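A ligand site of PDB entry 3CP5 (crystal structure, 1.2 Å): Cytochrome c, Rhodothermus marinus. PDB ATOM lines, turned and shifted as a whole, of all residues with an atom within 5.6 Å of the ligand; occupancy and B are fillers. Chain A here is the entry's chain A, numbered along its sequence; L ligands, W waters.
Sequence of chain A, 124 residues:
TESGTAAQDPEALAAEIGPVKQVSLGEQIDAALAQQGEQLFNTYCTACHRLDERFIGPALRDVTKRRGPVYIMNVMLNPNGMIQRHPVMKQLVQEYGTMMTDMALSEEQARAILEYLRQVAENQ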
ATOM      1  N   PHE A  41     -19.898  -7.687 -35.005  1.00  0.00           N
ATOM      2  CA  PHE A  41     -20.087  -8.043 -33.611  1.00  0.00           C
ATOM      3  C   PHE A  41     -20.794  -9.398 -33.504  1.00  0.00           C
ATOM      4  O   PHE A  41     -20.430 -10.247 -32.710  1.00  0.00           O
ATOM      5  CB  PHE A  41     -20.849  -6.935 -32.893  1.00  0.00           C
ATOM      6  CG  PHE A  41     -20.980  -7.105 -31.392  1.00  0.00           C
ATOM      7  CD1 PHE A  41     -20.062  -6.574 -30.508  1.00  0.00           C
ATOM      8  CD2 PHE A  41     -22.058  -7.824 -30.868  1.00  0.00           C
ATOM      9  CE1 PHE A  41     -20.162  -6.710 -29.156  1.00  0.00           C
ATOM     10  CE2 PHE A  41     -22.147  -7.981 -29.515  1.00  0.00           C
ATOM     11  CZ  PHE A  41     -21.223  -7.456 -28.658  1.00  0.00           C
ATOM     12  N   TYR A  44     -18.046 -12.074 -34.524  1.00  0.00           N
ATOM     13  CA  TYR A  44     -16.868 -12.220 -33.696  1.00  0.00           C
ATOM     14  C   TYR A  44     -17.118 -12.185 -32.187  1.00  0.00           C
ATOM     15  O   TYR A  44     -16.247 -12.705 -31.448  1.00  0.00           O
ATOM     16  CB  TYR A  44     -15.829 -11.149 -34.025  1.00  0.00           C
ATOM     17  CG  TYR A  44     -15.058 -11.255 -35.304  1.00  0.00           C
ATOM     18  CD1 TYR A  44     -15.496 -10.757 -36.515  1.00  0.00           C
ATOM     19  CD2 TYR A  44     -13.808 -11.878 -35.328  1.00  0.00           C
ATOM     20  CE1 TYR A  44     -14.753 -10.887 -37.677  1.00  0.00           C
ATOM     21  CE2 TYR A  44     -13.057 -11.989 -36.477  1.00  0.00           C
ATOM     22  CZ  TYR A  44     -13.533 -11.498 -37.673  1.00  0.00           C
ATOM     23  OH  TYR A  44     -12.801 -11.583 -38.840  1.00  0.00           O
ATOM     24  N   CYS A  45     -18.189 -11.569 -31.725  1.00  0.00           N
ATOM     25  CA  CYS A  45     -18.263 -11.183 -30.325  1.00  0.00           C
ATOM     26  C   CYS A  45     -19.450 -11.773 -29.573  1.00  0.00           C
ATOM     27  O   CYS A  45     -19.319 -12.039 -28.345  1.00  0.00           O
ATOM     28  CB  CYS A  45     -18.340  -9.650 -30.183  1.00  0.00           C
ATOM     29  SG  CYS A  45     -17.252  -8.683 -31.258  1.00  0.00           S
ATOM     30  N   ALA A  47     -20.640 -14.683 -29.433  1.00  0.00           N
ATOM     31  CA  ALA A  47     -20.402 -15.983 -28.837  1.00  0.00           C
ATOM     32  C   ALA A  47     -20.115 -15.855 -27.339  1.00  0.00           C
ATOM     33  O   ALA A  47     -20.350 -16.790 -26.595  1.00  0.00           O
ATOM     34  CB  ALA A  47     -19.216 -16.645 -29.530  1.00  0.00           C
ATOM     35  N   CYS A  48     -19.550 -14.709 -26.905  1.00  0.00           N
ATOM     36  CA  CYS A  48     -19.161 -14.563 -25.535  1.00  0.00           C
ATOM     37  C   CYS A  48     -19.773 -13.368 -24.823  1.00  0.00           C
ATOM     38  O   CYS A  48     -19.784 -13.325 -23.570  1.00  0.00           O
ATOM     39  CB  CYS A  48     -17.623 -14.394 -25.434  1.00  0.00           C
ATOM     40  SG  CYS A  48     -16.732 -15.869 -25.996  1.00  0.00           S
ATOM     41  N   HIS A  49     -20.275 -12.362 -25.536  1.00  0.00           N
ATOM     42  CA  HIS A  49     -20.774 -11.156 -24.925  1.00  0.00           C
ATOM     43  C   HIS A  49     -22.222 -10.876 -25.297  1.00  0.00           C
ATOM     44  O   HIS A  49     -22.584 -11.086 -26.460  1.00  0.00           O
ATOM     45  CB  HIS A  49     -19.940  -9.947 -25.363  1.00  0.00           C
ATOM     46  CG  HIS A  49     -18.533  -9.816 -24.891  1.00  0.00           C
ATOM     47  ND1 HIS A  49     -18.187  -9.340 -23.633  1.00  0.00           N
ATOM     48  CD2 HIS A  49     -17.348 -10.050 -25.551  1.00  0.00           C
ATOM     49  CE1 HIS A  49     -16.842  -9.314 -23.547  1.00  0.00           C
ATOM     50  NE2 HIS A  49     -16.318  -9.755 -24.693  1.00  0.00           N
ATOM     51  N   ILE A  56     -20.207 -15.065 -21.020  1.00  0.00           N
ATOM     52  CA  ILE A  56     -18.850 -15.573 -20.843  1.00  0.00           C
ATOM     53  C   ILE A  56     -17.933 -14.435 -20.495  1.00  0.00           C
ATOM     54  O   ILE A  56     -17.068 -14.580 -19.646  1.00  0.00           O
ATOM     55  CB  ILE A  56     -18.377 -16.368 -22.079  1.00  0.00           C
ATOM     56  CG1 ILE A  56     -19.226 -17.639 -22.248  1.00  0.00           C
ATOM     57  CG2 ILE A  56     -16.885 -16.644 -22.040  1.00  0.00           C
ATOM     58  CD1 ILE A  56     -19.115 -18.340 -23.584  1.00  0.00           C
ATOM     59  N   GLY A  57     -18.172 -13.285 -21.110  1.00  0.00           N
ATOM     60  CA  GLY A  57     -17.485 -12.059 -20.740  1.00  0.00           C
ATOM     61  C   GLY A  57     -18.460 -11.012 -20.230  1.00  0.00           C
ATOM     62  O   GLY A  57     -19.677 -11.241 -20.181  1.00  0.00           O
ATOM     63  N   PRO A  58     -17.960  -9.832 -19.871  1.00  0.00           N
ATOM     64  CA  PRO A  58     -18.841  -8.767 -19.350  1.00  0.00           C
ATOM     65  C   PRO A  58     -19.831  -8.193 -20.339  1.00  0.00           C
ATOM     66  O   PRO A  58     -19.644  -8.256 -21.559  1.00  0.00           O
ATOM     67  CB  PRO A  58     -17.846  -7.697 -18.908  1.00  0.00           C
ATOM     68  CG  PRO A  58     -16.573  -7.986 -19.610  1.00  0.00           C
ATOM     69  CD  PRO A  58     -16.550  -9.469 -19.851  1.00  0.00           C
ATOM     70  N   ALA A  59     -20.911  -7.581 -19.840  1.00  0.00           N
ATOM     71  CA  ALA A  59     -21.849  -6.838 -20.645  1.00  0.00           C
ATOM     72  C   ALA A  59     -21.175  -5.667 -21.307  1.00  0.00           C
ATOM     73  O   ALA A  59     -20.335  -4.975 -20.715  1.00  0.00           O
ATOM     74  CB  ALA A  59     -22.978  -6.311 -19.746  1.00  0.00           C
ATOM     75  N   LEU A  60     -21.540  -5.362 -22.547  1.00  0.00           N
ATOM     76  CA  LEU A  60     -20.890  -4.353 -23.335  1.00  0.00           C
ATOM     77  C   LEU A  60     -21.673  -3.108 -23.693  1.00  0.00           C
ATOM     78  O   LEU A  60     -21.056  -2.191 -24.267  1.00  0.00           O
ATOM     79  CB  LEU A  60     -20.197  -4.902 -24.595  1.00  0.00           C
ATOM     80  CG  LEU A  60     -19.095  -5.954 -24.351  1.00  0.00           C
ATOM     81  CD1 LEU A  60     -18.578  -6.460 -25.693  1.00  0.00           C
ATOM     82  CD2 LEU A  60     -17.964  -5.423 -23.491  1.00  0.00           C
ATOM     83  N   VAL A  63     -19.882  -0.016 -22.576  1.00  0.00           N
ATOM     84  CA  VAL A  63     -18.385  -0.019 -22.528  1.00  0.00           C
ATOM     85  C   VAL A  63     -17.798   1.287 -23.025  1.00  0.00           C
ATOM     86  O   VAL A  63     -16.780   1.717 -22.459  1.00  0.00           O
ATOM     87  CB  VAL A  63     -17.817  -1.244 -23.253  1.00  0.00           C
ATOM     88  CG1 VAL A  63     -17.887  -1.160 -24.760  1.00  0.00           C
ATOM     89  CG2 VAL A  63     -16.383  -1.446 -22.775  1.00  0.00           C
ATOM     90  N   ARG A  67     -15.027   3.144 -20.642  1.00  0.00           N
ATOM     91  CA  ARG A  67     -13.686   3.011 -21.183  1.00  0.00           C
ATOM     92  C   ARG A  67     -13.464   3.889 -22.365  1.00  0.00           C
ATOM     93  O   ARG A  67     -14.411   4.153 -23.089  1.00  0.00           O
ATOM     94  CB  ARG A  67     -13.469   1.572 -21.662  1.00  0.00           C
ATOM     95  CG  ARG A  67     -13.822   0.471 -20.679  1.00  0.00           C
ATOM     96  CD  ARG A  67     -12.928   0.419 -19.434  1.00  0.00           C
ATOM     97  NE  ARG A  67     -13.370  -0.708 -18.601  1.00  0.00           N
ATOM     98  CZ  ARG A  67     -13.527  -0.791 -17.311  1.00  0.00           C
ATOM     99  NH1 ARG A  67     -13.253   0.224 -16.532  1.00  0.00           N
ATOM    100  NH2 ARG A  67     -13.977  -1.925 -16.812  1.00  0.00           N
ATOM    101  N   TYR A  71      -8.457   1.980 -25.554  1.00  0.00           N
ATOM    102  CA  TYR A  71      -8.594   0.731 -24.807  1.00  0.00           C
ATOM    103  C   TYR A  71      -9.466  -0.268 -25.517  1.00  0.00           C
ATOM    104  O   TYR A  71      -9.104  -1.425 -25.629  1.00  0.00           O
ATOM    105  CB  TYR A  71      -9.129   1.027 -23.394  1.00  0.00           C
ATOM    106  CG  TYR A  71      -9.471  -0.175 -22.534  1.00  0.00           C
ATOM    107  CD1 TYR A  71      -8.526  -0.733 -21.679  1.00  0.00           C
ATOM    108  CD2 TYR A  71     -10.719  -0.761 -22.563  1.00  0.00           C
ATOM    109  CE1 TYR A  71      -8.871  -1.835 -20.902  1.00  0.00           C
ATOM    110  CE2 TYR A  71     -11.090  -1.831 -21.800  1.00  0.00           C
ATOM    111  CZ  TYR A  71     -10.154  -2.371 -20.958  1.00  0.00           C
ATOM    112  OH  TYR A  71     -10.488  -3.457 -20.182  1.00  0.00           O
ATOM    113  N   ILE A  72     -10.654   0.140 -25.952  1.00  0.00           N
ATOM    114  CA  ILE A  72     -11.555  -0.832 -26.541  1.00  0.00           C
ATOM    115  C   ILE A  72     -10.978  -1.407 -27.838  1.00  0.00           C
ATOM    116  O   ILE A  72     -11.064  -2.606 -28.063  1.00  0.00           O
ATOM    117  CB  ILE A  72     -12.910  -0.166 -26.797  1.00  0.00           C
ATOM    118  CG1 ILE A  72     -13.596   0.229 -25.472  1.00  0.00           C
ATOM    119  CG2 ILE A  72     -13.851  -1.053 -27.616  1.00  0.00           C
ATOM    120  CD1 ILE A  72     -14.750   1.211 -25.646  1.00  0.00           C
ATOM    121  N   VAL A  75      -8.118  -3.978 -26.876  1.00  0.00           N
ATOM    122  CA  VAL A  75      -8.662  -5.241 -26.363  1.00  0.00           C
ATOM    123  C   VAL A  75      -9.073  -6.130 -27.531  1.00  0.00           C
ATOM    124  O   VAL A  75      -8.776  -7.322 -27.546  1.00  0.00           O
ATOM    125  CB  VAL A  75      -9.839  -5.002 -25.390  1.00  0.00           C
ATOM    126  CG1 VAL A  75     -10.560  -6.303 -25.127  1.00  0.00           C
ATOM    127  CG2 VAL A  75      -9.376  -4.387 -24.075  1.00  0.00           C
ATOM    128  N   MET A  76      -9.744  -5.572 -28.558  1.00  0.00           N
ATOM    129  CA  MET A  76     -10.122  -6.335 -29.737  1.00  0.00           C
ATOM    130  C   MET A  76      -8.943  -6.834 -30.572  1.00  0.00           C
ATOM    131  O   MET A  76      -8.931  -8.003 -31.033  1.00  0.00           O
ATOM    132  CB  MET A  76     -11.055  -5.487 -30.661  1.00  0.00           C
ATOM    133  CG  MET A  76     -12.467  -5.314 -30.146  1.00  0.00           C
ATOM    134  SD  MET A  76     -13.448  -4.546 -31.487  1.00  0.00           S
ATOM    135  CE  MET A  76     -13.516  -2.830 -30.981  1.00  0.00           C
ATOM    136  N   ILE A  83      -4.196  -8.248 -21.693  1.00  0.00           N
ATOM    137  CA  ILE A  83      -4.303  -9.063 -20.498  1.00  0.00           C
ATOM    138  C   ILE A  83      -2.967  -9.081 -19.779  1.00  0.00           C
ATOM    139  O   ILE A  83      -2.931  -9.087 -18.549  1.00  0.00           O
ATOM    140  CB  ILE A  83      -4.757 -10.516 -20.874  1.00  0.00           C
ATOM    141  CG1 ILE A  83      -6.226 -10.522 -21.262  1.00  0.00           C
ATOM    142  CG2 ILE A  83      -4.410 -11.464 -19.764  1.00  0.00           C
ATOM    143  CD1 ILE A  83      -6.706 -11.706 -22.024  1.00  0.00           C
ATOM    144  N   VAL A  88      -6.861  -3.242 -15.879  1.00  0.00           N
ATOM    145  CA  VAL A  88      -8.284  -3.483 -15.914  1.00  0.00           C
ATOM    146  C   VAL A  88      -8.605  -4.845 -16.524  1.00  0.00           C
ATOM    147  O   VAL A  88      -9.439  -5.587 -16.033  1.00  0.00           O
ATOM    148  CB  VAL A  88      -8.945  -2.359 -16.707  1.00  0.00           C
ATOM    149  CG1 VAL A  88     -10.395  -2.648 -16.902  1.00  0.00           C
ATOM    150  CG2 VAL A  88      -8.713  -1.037 -15.946  1.00  0.00           C
ATOM    151  N   MET A  89      -7.909  -5.177 -17.645  1.00  0.00           N
ATOM    152  CA  MET A  89      -8.090  -6.495 -18.268  1.00  0.00           C
ATOM    153  C   MET A  89      -7.585  -7.610 -17.374  1.00  0.00           C
ATOM    154  O   MET A  89      -8.164  -8.699 -17.302  1.00  0.00           O
ATOM    155  CB  MET A  89      -7.437  -6.591 -19.652  1.00  0.00           C
ATOM    156  CG  MET A  89      -8.244  -5.997 -20.780  1.00  0.00           C
ATOM    157  SD  MET A  89      -9.735  -6.928 -21.163  1.00  0.00           S
ATOM    158  CE  MET A  89      -9.206  -8.296 -22.170  1.00  0.00           C
ATOM    159  N   LEU A  92     -10.281  -8.320 -14.889  1.00  0.00           N
ATOM    160  CA  LEU A  92     -11.408  -9.034 -15.523  1.00  0.00           C
ATOM    161  C   LEU A  92     -11.090 -10.490 -15.780  1.00  0.00           C
ATOM    162  O   LEU A  92     -12.027 -11.320 -15.674  1.00  0.00           O
ATOM    163  CB  LEU A  92     -11.802  -8.256 -16.785  1.00  0.00           C
ATOM    164  CG  LEU A  92     -12.463  -6.895 -16.612  1.00  0.00           C
ATOM    165  CD1 LEU A  92     -12.597  -6.179 -17.946  1.00  0.00           C
ATOM    166  CD2 LEU A  92     -13.890  -7.073 -16.089  1.00  0.00           C
ATOM    167  N   VAL A  93      -9.845 -10.820 -16.123  1.00  0.00           N
ATOM    168  CA  VAL A  93      -9.518 -12.253 -16.242  1.00  0.00           C
ATOM    169  C   VAL A  93      -9.688 -12.939 -14.905  1.00  0.00           C
ATOM    170  O   VAL A  93     -10.183 -14.080 -14.839  1.00  0.00           O
ATOM    171  CB  VAL A  93      -8.087 -12.467 -16.789  1.00  0.00           C
ATOM    172  CG1 VAL A  93      -7.679 -13.915 -16.677  1.00  0.00           C
ATOM    173  CG2 VAL A  93      -7.977 -12.028 -18.227  1.00  0.00           C
ATOM    174  N   TYR A  96     -13.563 -13.404 -14.579  1.00  0.00           N
ATOM    175  CA  TYR A  96     -14.297 -14.165 -15.562  1.00  0.00           C
ATOM    176  C   TYR A  96     -13.688 -15.504 -15.842  1.00  0.00           C
ATOM    177  O   TYR A  96     -14.406 -16.408 -16.299  1.00  0.00           O
ATOM    178  CB  TYR A  96     -14.437 -13.355 -16.867  1.00  0.00           C
ATOM    179  CG  TYR A  96     -15.551 -12.340 -16.666  1.00  0.00           C
ATOM    180  CD1 TYR A  96     -16.883 -12.620 -16.932  1.00  0.00           C
ATOM    181  CD2 TYR A  96     -15.296 -11.071 -16.178  1.00  0.00           C
ATOM    182  CE1 TYR A  96     -17.880 -11.681 -16.723  1.00  0.00           C
ATOM    183  CE2 TYR A  96     -16.303 -10.136 -15.978  1.00  0.00           C
ATOM    184  CZ  TYR A  96     -17.621 -10.428 -16.253  1.00  0.00           C
ATOM    185  OH  TYR A  96     -18.645  -9.531 -16.057  1.00  0.00           O
ATOM    186  N   GLY A  97     -12.402 -15.641 -15.608  1.00  0.00           N
ATOM    187  CA  GLY A  97     -11.718 -16.929 -15.681  1.00  0.00           C
ATOM    188  C   GLY A  97     -11.216 -17.299 -17.056  1.00  0.00           C
ATOM    189  O   GLY A  97     -10.052 -17.566 -17.357  1.00  0.00           O
ATOM    190  N   THR A  98     -12.097 -17.321 -18.013  1.00  0.00           N
ATOM    191  CA  THR A  98     -11.636 -17.560 -19.389  1.00  0.00           C
ATOM    192  C   THR A  98     -10.989 -16.315 -19.984  1.00  0.00           C
ATOM    193  O   THR A  98     -11.143 -15.200 -19.478  1.00  0.00           O
ATOM    194  CB  THR A  98     -12.844 -18.031 -20.200  1.00  0.00           C
ATOM    195  OG1 THR A  98     -13.762 -16.961 -20.269  1.00  0.00           O
ATOM    196  CG2 THR A  98     -13.444 -19.232 -19.499  1.00  0.00           C
ATOM    197  N   MET A  99     -10.257 -16.511 -21.104  1.00  0.00           N
ATOM    198  CA  MET A  99      -9.544 -15.407 -21.734  1.00  0.00           C
ATOM    199  C   MET A  99     -10.085 -15.125 -23.130  1.00  0.00           C
ATOM    200  O   MET A  99     -10.465 -15.984 -23.910  1.00  0.00           O
ATOM    201  CB  MET A  99      -8.043 -15.692 -21.757  1.00  0.00           C
ATOM    202  CG  MET A  99      -7.366 -15.914 -20.400  1.00  0.00           C
ATOM    203  SD  MET A  99      -5.592 -15.883 -20.517  1.00  0.00           S
ATOM    204  CE  MET A  99      -5.256 -17.140 -21.759  1.00  0.00           C
ATOM    205  N   MET A 100     -10.093 -13.850 -23.428  1.00  0.00           N
ATOM    206  CA  MET A 100     -10.306 -13.351 -24.779  1.00  0.00           C
ATOM    207  C   MET A 100      -9.052 -13.617 -25.602  1.00  0.00           C
ATOM    208  O   MET A 100      -7.972 -13.385 -25.029  1.00  0.00           O
ATOM    209  CB  MET A 100     -10.626 -11.887 -24.687  1.00  0.00           C
ATOM    210  CG  MET A 100     -11.353 -11.342 -25.829  1.00  0.00           C
ATOM    211  SD  MET A 100     -12.042  -9.702 -25.508  1.00  0.00           S
ATOM    212  CE  MET A 100     -11.825  -9.154 -27.242  1.00  0.00           C
ATOM    213  N   THR A 101      -9.110 -14.084 -26.822  1.00  0.00           N
ATOM    214  CA  THR A 101      -7.881 -14.392 -27.567  1.00  0.00           C
ATOM    215  C   THR A 101      -7.934 -13.791 -28.969  1.00  0.00           C
ATOM    216  O   THR A 101      -8.986 -13.336 -29.403  1.00  0.00           O
ATOM    217  CB  THR A 101      -7.595 -15.885 -27.765  1.00  0.00           C
ATOM    218  OG1 THR A 101      -8.716 -16.503 -28.396  1.00  0.00           O
ATOM    219  CG2 THR A 101      -7.348 -16.547 -26.407  1.00  0.00           C
ATOM    220  N   MET A 103      -8.295 -12.929 -32.636  1.00  0.00           N
ATOM    221  CA  MET A 103      -9.285 -13.235 -33.661  1.00  0.00           C
ATOM    222  C   MET A 103      -8.906 -12.872 -35.056  1.00  0.00           C
ATOM    223  O   MET A 103      -9.664 -12.962 -36.006  1.00  0.00           O
ATOM    224  CB  MET A 103     -10.626 -12.567 -33.283  1.00  0.00           C
ATOM    225  CG  MET A 103     -11.227 -13.131 -32.031  1.00  0.00           C
ATOM    226  SD  MET A 103     -12.436 -12.021 -31.257  1.00  0.00           S
ATOM    227  CE  MET A 103     -11.249 -10.813 -30.621  1.00  0.00           C
ATOM    228  N   LEU A 105      -8.331  -9.952 -36.245  1.00  0.00           N
ATOM    229  CA  LEU A 105      -9.051  -8.756 -36.666  1.00  0.00           C
ATOM    230  C   LEU A 105      -8.109  -7.670 -37.185  1.00  0.00           C
ATOM    231  O   LEU A 105      -6.984  -7.526 -36.724  1.00  0.00           O
ATOM    232  CB  LEU A 105      -9.795  -8.133 -35.465  1.00  0.00           C
ATOM    233  CG  LEU A 105     -11.106  -8.794 -35.084  1.00  0.00           C
ATOM    234  CD1 LEU A 105     -11.452  -8.390 -33.665  1.00  0.00           C
ATOM    235  CD2 LEU A 105     -12.205  -8.601 -36.067  1.00  0.00           C
ATOM    236  N   ILE A 113     -16.662  -2.055 -35.342  1.00  0.00           N
ATOM    237  CA  ILE A 113     -17.244  -2.572 -34.119  1.00  0.00           C
ATOM    238  C   ILE A 113     -17.318  -1.471 -33.078  1.00  0.00           C
ATOM    239  O   ILE A 113     -18.346  -1.318 -32.384  1.00  0.00           O
ATOM    240  CB  ILE A 113     -16.516  -3.832 -33.607  1.00  0.00           C
ATOM    241  CG1 ILE A 113     -16.644  -4.979 -34.620  1.00  0.00           C
ATOM    242  CG2 ILE A 113     -17.012  -4.245 -32.244  1.00  0.00           C
ATOM    243  CD1 ILE A 113     -15.790  -6.180 -34.314  1.00  0.00           C
ATOM    244  N   LEU A 117     -20.616  -0.097 -31.048  1.00  0.00           N
ATOM    245  CA  LEU A 117     -20.642   0.078 -29.606  1.00  0.00           C
ATOM    246  C   LEU A 117     -21.043   1.490 -29.180  1.00  0.00           C
ATOM    247  O   LEU A 117     -21.780   1.696 -28.235  1.00  0.00           O
ATOM    248  CB  LEU A 117     -19.339  -0.396 -28.958  1.00  0.00           C
ATOM    249  CG  LEU A 117     -19.047  -1.889 -29.057  1.00  0.00           C
ATOM    250  CD1 LEU A 117     -17.621  -2.176 -28.622  1.00  0.00           C
ATOM    251  CD2 LEU A 117     -19.999  -2.704 -28.199  1.00  0.00           C
HETATM  252 FE1  LIG L   1     -14.343  -9.764 -25.154  1.00  0.00          FE
HETATM  253  C1  LIG L   1     -13.477  -8.495 -22.095  1.00  0.00           C
HETATM  254  C2  LIG L   1     -14.820  -6.611 -26.357  1.00  0.00           C
HETATM  255  C3  LIG L   1     -14.872 -11.077 -28.278  1.00  0.00           C
HETATM  256  C4  LIG L   1     -14.454 -12.881 -23.825  1.00  0.00           C
HETATM  257  N1  LIG L   1     -14.205  -7.943 -24.369  1.00  0.00           N
HETATM  258  C5  LIG L   1     -13.762  -7.577 -23.094  1.00  0.00           C
HETATM  259  C6  LIG L   1     -13.656  -6.136 -23.021  1.00  0.00           C
HETATM  260  C7  LIG L   1     -14.053  -5.615 -24.198  1.00  0.00           C
HETATM  261  C8  LIG L   1     -14.365  -6.755 -25.041  1.00  0.00           C
HETATM  262  C9  LIG L   1     -14.161  -4.130 -24.596  1.00  0.00           C
HETATM  263  C10 LIG L   1     -13.327  -5.306 -21.757  1.00  0.00           C
HETATM  264  C11 LIG L   1     -14.572  -4.885 -20.973  1.00  0.00           C
HETATM  265  C12 LIG L   1     -14.279  -3.885 -19.881  1.00  0.00           C
HETATM  266  O1  LIG L   1     -15.203  -3.679 -19.025  1.00  0.00           O
HETATM  267  O2  LIG L   1     -13.177  -3.277 -19.885  1.00  0.00           O
HETATM  268  N2  LIG L   1     -14.811  -9.025 -26.946  1.00  0.00           N
HETATM  269  C13 LIG L   1     -15.096  -7.702 -27.201  1.00  0.00           C
HETATM  270  C14 LIG L   1     -15.450  -7.550 -28.591  1.00  0.00           C
HETATM  271  C15 LIG L   1     -15.400  -8.778 -29.186  1.00  0.00           C
HETATM  272  C16 LIG L   1     -14.996  -9.697 -28.136  1.00  0.00           C
HETATM  273  C17 LIG L   1     -15.837  -6.187 -29.207  1.00  0.00           C
HETATM  274  C18 LIG L   1     -15.522  -9.119 -30.680  1.00  0.00           C
HETATM  275  C19 LIG L   1     -14.606  -8.440 -31.517  1.00  0.00           C
HETATM  276  N3  LIG L   1     -14.535 -11.606 -25.910  1.00  0.00           N
HETATM  277  C20 LIG L   1     -14.715 -11.972 -27.240  1.00  0.00           C
HETATM  278  C21 LIG L   1     -14.812 -13.423 -27.353  1.00  0.00           C
HETATM  279  C22 LIG L   1     -14.700 -13.937 -26.120  1.00  0.00           C
HETATM  280  C23 LIG L   1     -14.593 -12.816 -25.218  1.00  0.00           C
HETATM  281  C24 LIG L   1     -15.233 -14.108 -28.649  1.00  0.00           C
HETATM  282  C25 LIG L   1     -14.972 -15.396 -25.656  1.00  0.00           C
HETATM  283  C26 LIG L   1     -14.135 -16.356 -26.285  1.00  0.00           C
HETATM  284  N4  LIG L   1     -14.006 -10.515 -23.331  1.00  0.00           N
HETATM  285  C27 LIG L   1     -14.126 -11.854 -22.976  1.00  0.00           C
HETATM  286  C28 LIG L   1     -13.842 -11.989 -21.539  1.00  0.00           C
HETATM  287  C29 LIG L   1     -13.462 -10.791 -21.102  1.00  0.00           C
HETATM  288  C30 LIG L   1     -13.658  -9.857 -22.203  1.00  0.00           C
HETATM  289  C31 LIG L   1     -13.883 -13.376 -20.849  1.00  0.00           C
HETATM  290  C32 LIG L   1     -12.925 -10.368 -19.728  1.00  0.00           C
HETATM  291  C33 LIG L   1     -11.373 -10.402 -19.735  1.00  0.00           C
HETATM  292  C34 LIG L   1     -10.911 -11.817 -19.997  1.00  0.00           C
HETATM  293  O3  LIG L   1     -10.223 -12.065 -21.034  1.00  0.00           O
HETATM  294  O4  LIG L   1     -11.280 -12.684 -19.120  1.00  0.00           O
HETATM  295  O   HOH W   1     -16.830  -4.836 -17.213  1.00  0.00           O
HETATM  296  O   HOH W   2     -14.430 -14.831 -31.971  1.00  0.00           O
HETATM  297  O   HOH W   3     -11.558 -13.976 -28.198  1.00  0.00           O
HETATM  298  O   HOH W   4     -13.460 -16.638 -22.923  1.00  0.00           O
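The side-chain sulfur of Cys 48 is covalently linked to a carbon (C25) of the ligand (1.9 Å).
The side-chain sulfur (SG) of Cys 45 is covalently linked to a carbon (C18) of the ligand, 1.9 Å away.
An iron atom (FE1) of the ligand is bound by a ring nitrogen (NE2) of His 49.
N of Met 100 sits at hydrogen-bond distance from O3 of the ligand, 3.0 Å away.
The side-chain sulfur (SD) of Met 100 is bound to an iron atom (FE1) of the ligand, at 2.3 Å.
The backbone carbonyl oxygen (O) of Thr 98 lies close to an oxygen (O4) of the ligand, at 2.5 Å.
OH of Tyr 71 lies within hydrogen-bond range of O2 of the ligand, at 2.7 Å.
The guanidinium group (NE) of Arg 67 lies within salt-bridge range of an oxygen (O2) of the ligand, 2.9 Å away.
The backbone NH (N) of Ile 56 is in hydrogen-bond range of the backbone carbonyl oxygen (O) of Cys 48 (3.1 Å).
O of Cys 48 sits at hydrogen-bond distance from N of Gly 57, at 2.9 Å.
O of Pro 58 sits at hydrogen-bond distance from ND1 of His 49 (2.8 Å).
The side-chain sulfur (SD) of Met 89 lies close to the side-chain hydroxyl (OH) of Tyr 71, 3.7 Å away.
Residues that only touch the ligand: Tyr 44 (3.3 Å), Val 93 (3.4 Å), Leu 92 (3.4 Å), Met 99 (3.5 Å), Pro 58 (3.6 Å), Met 76 (3.6 Å), Ile 56 (3.6 Å), Ile 83 (3.7 Å), Val 75 (3.7 Å), Gly 57 (3.7 Å), Ile 113 (3.8 Å), Leu 105 (3.8 Å), Leu 60 (3.8 Å), Met 89 (3.9 Å), Val 63 (3.9 Å), Tyr 96 (3.9 Å) and Met 103 (3.96 Å).
Hydrophobic or aromatic side chains within 4 Å of the ligand: Tyr 44, His 49, Pro 58, Leu 60, Val 63, Tyr 71, Val 75, Met 76, Ile 83, Met 89, Leu 92, Val 93, Tyr 96, Met 100, Met 103, Leu 105 and Ile 113.
24 residues have an atom within 4 Å of the ligand: Tyr 44, Cys 45, Cys 48, His 49, Ile 56, Gly 57, Pro 58, Leu 60, Val 63, Arg 67, Tyr 71, Val 75, Met 76, Ile 83, Met 89, Leu 92, Val 93, Tyr 96, Thr 98, Met 99, Met 100, Met 103, Leu 105 and Ile 113.
Water W4 lies within hydrogen-bond range of the side-chain hydroxyl (OG1) of Thr 98 (2.7 Å) and the backbone carbonyl oxygen (O) of Met 99 (3.2 Å).
Water W3 bridges the backbone NH (N) of Thr 101 (2.8 Å) and the side-chain sulfur (SD) of Met 103 (3.7 Å).
Water W2 bridges O of Tyr 44 (2.8 Å) and SD of Met 103 (3.5 Å).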
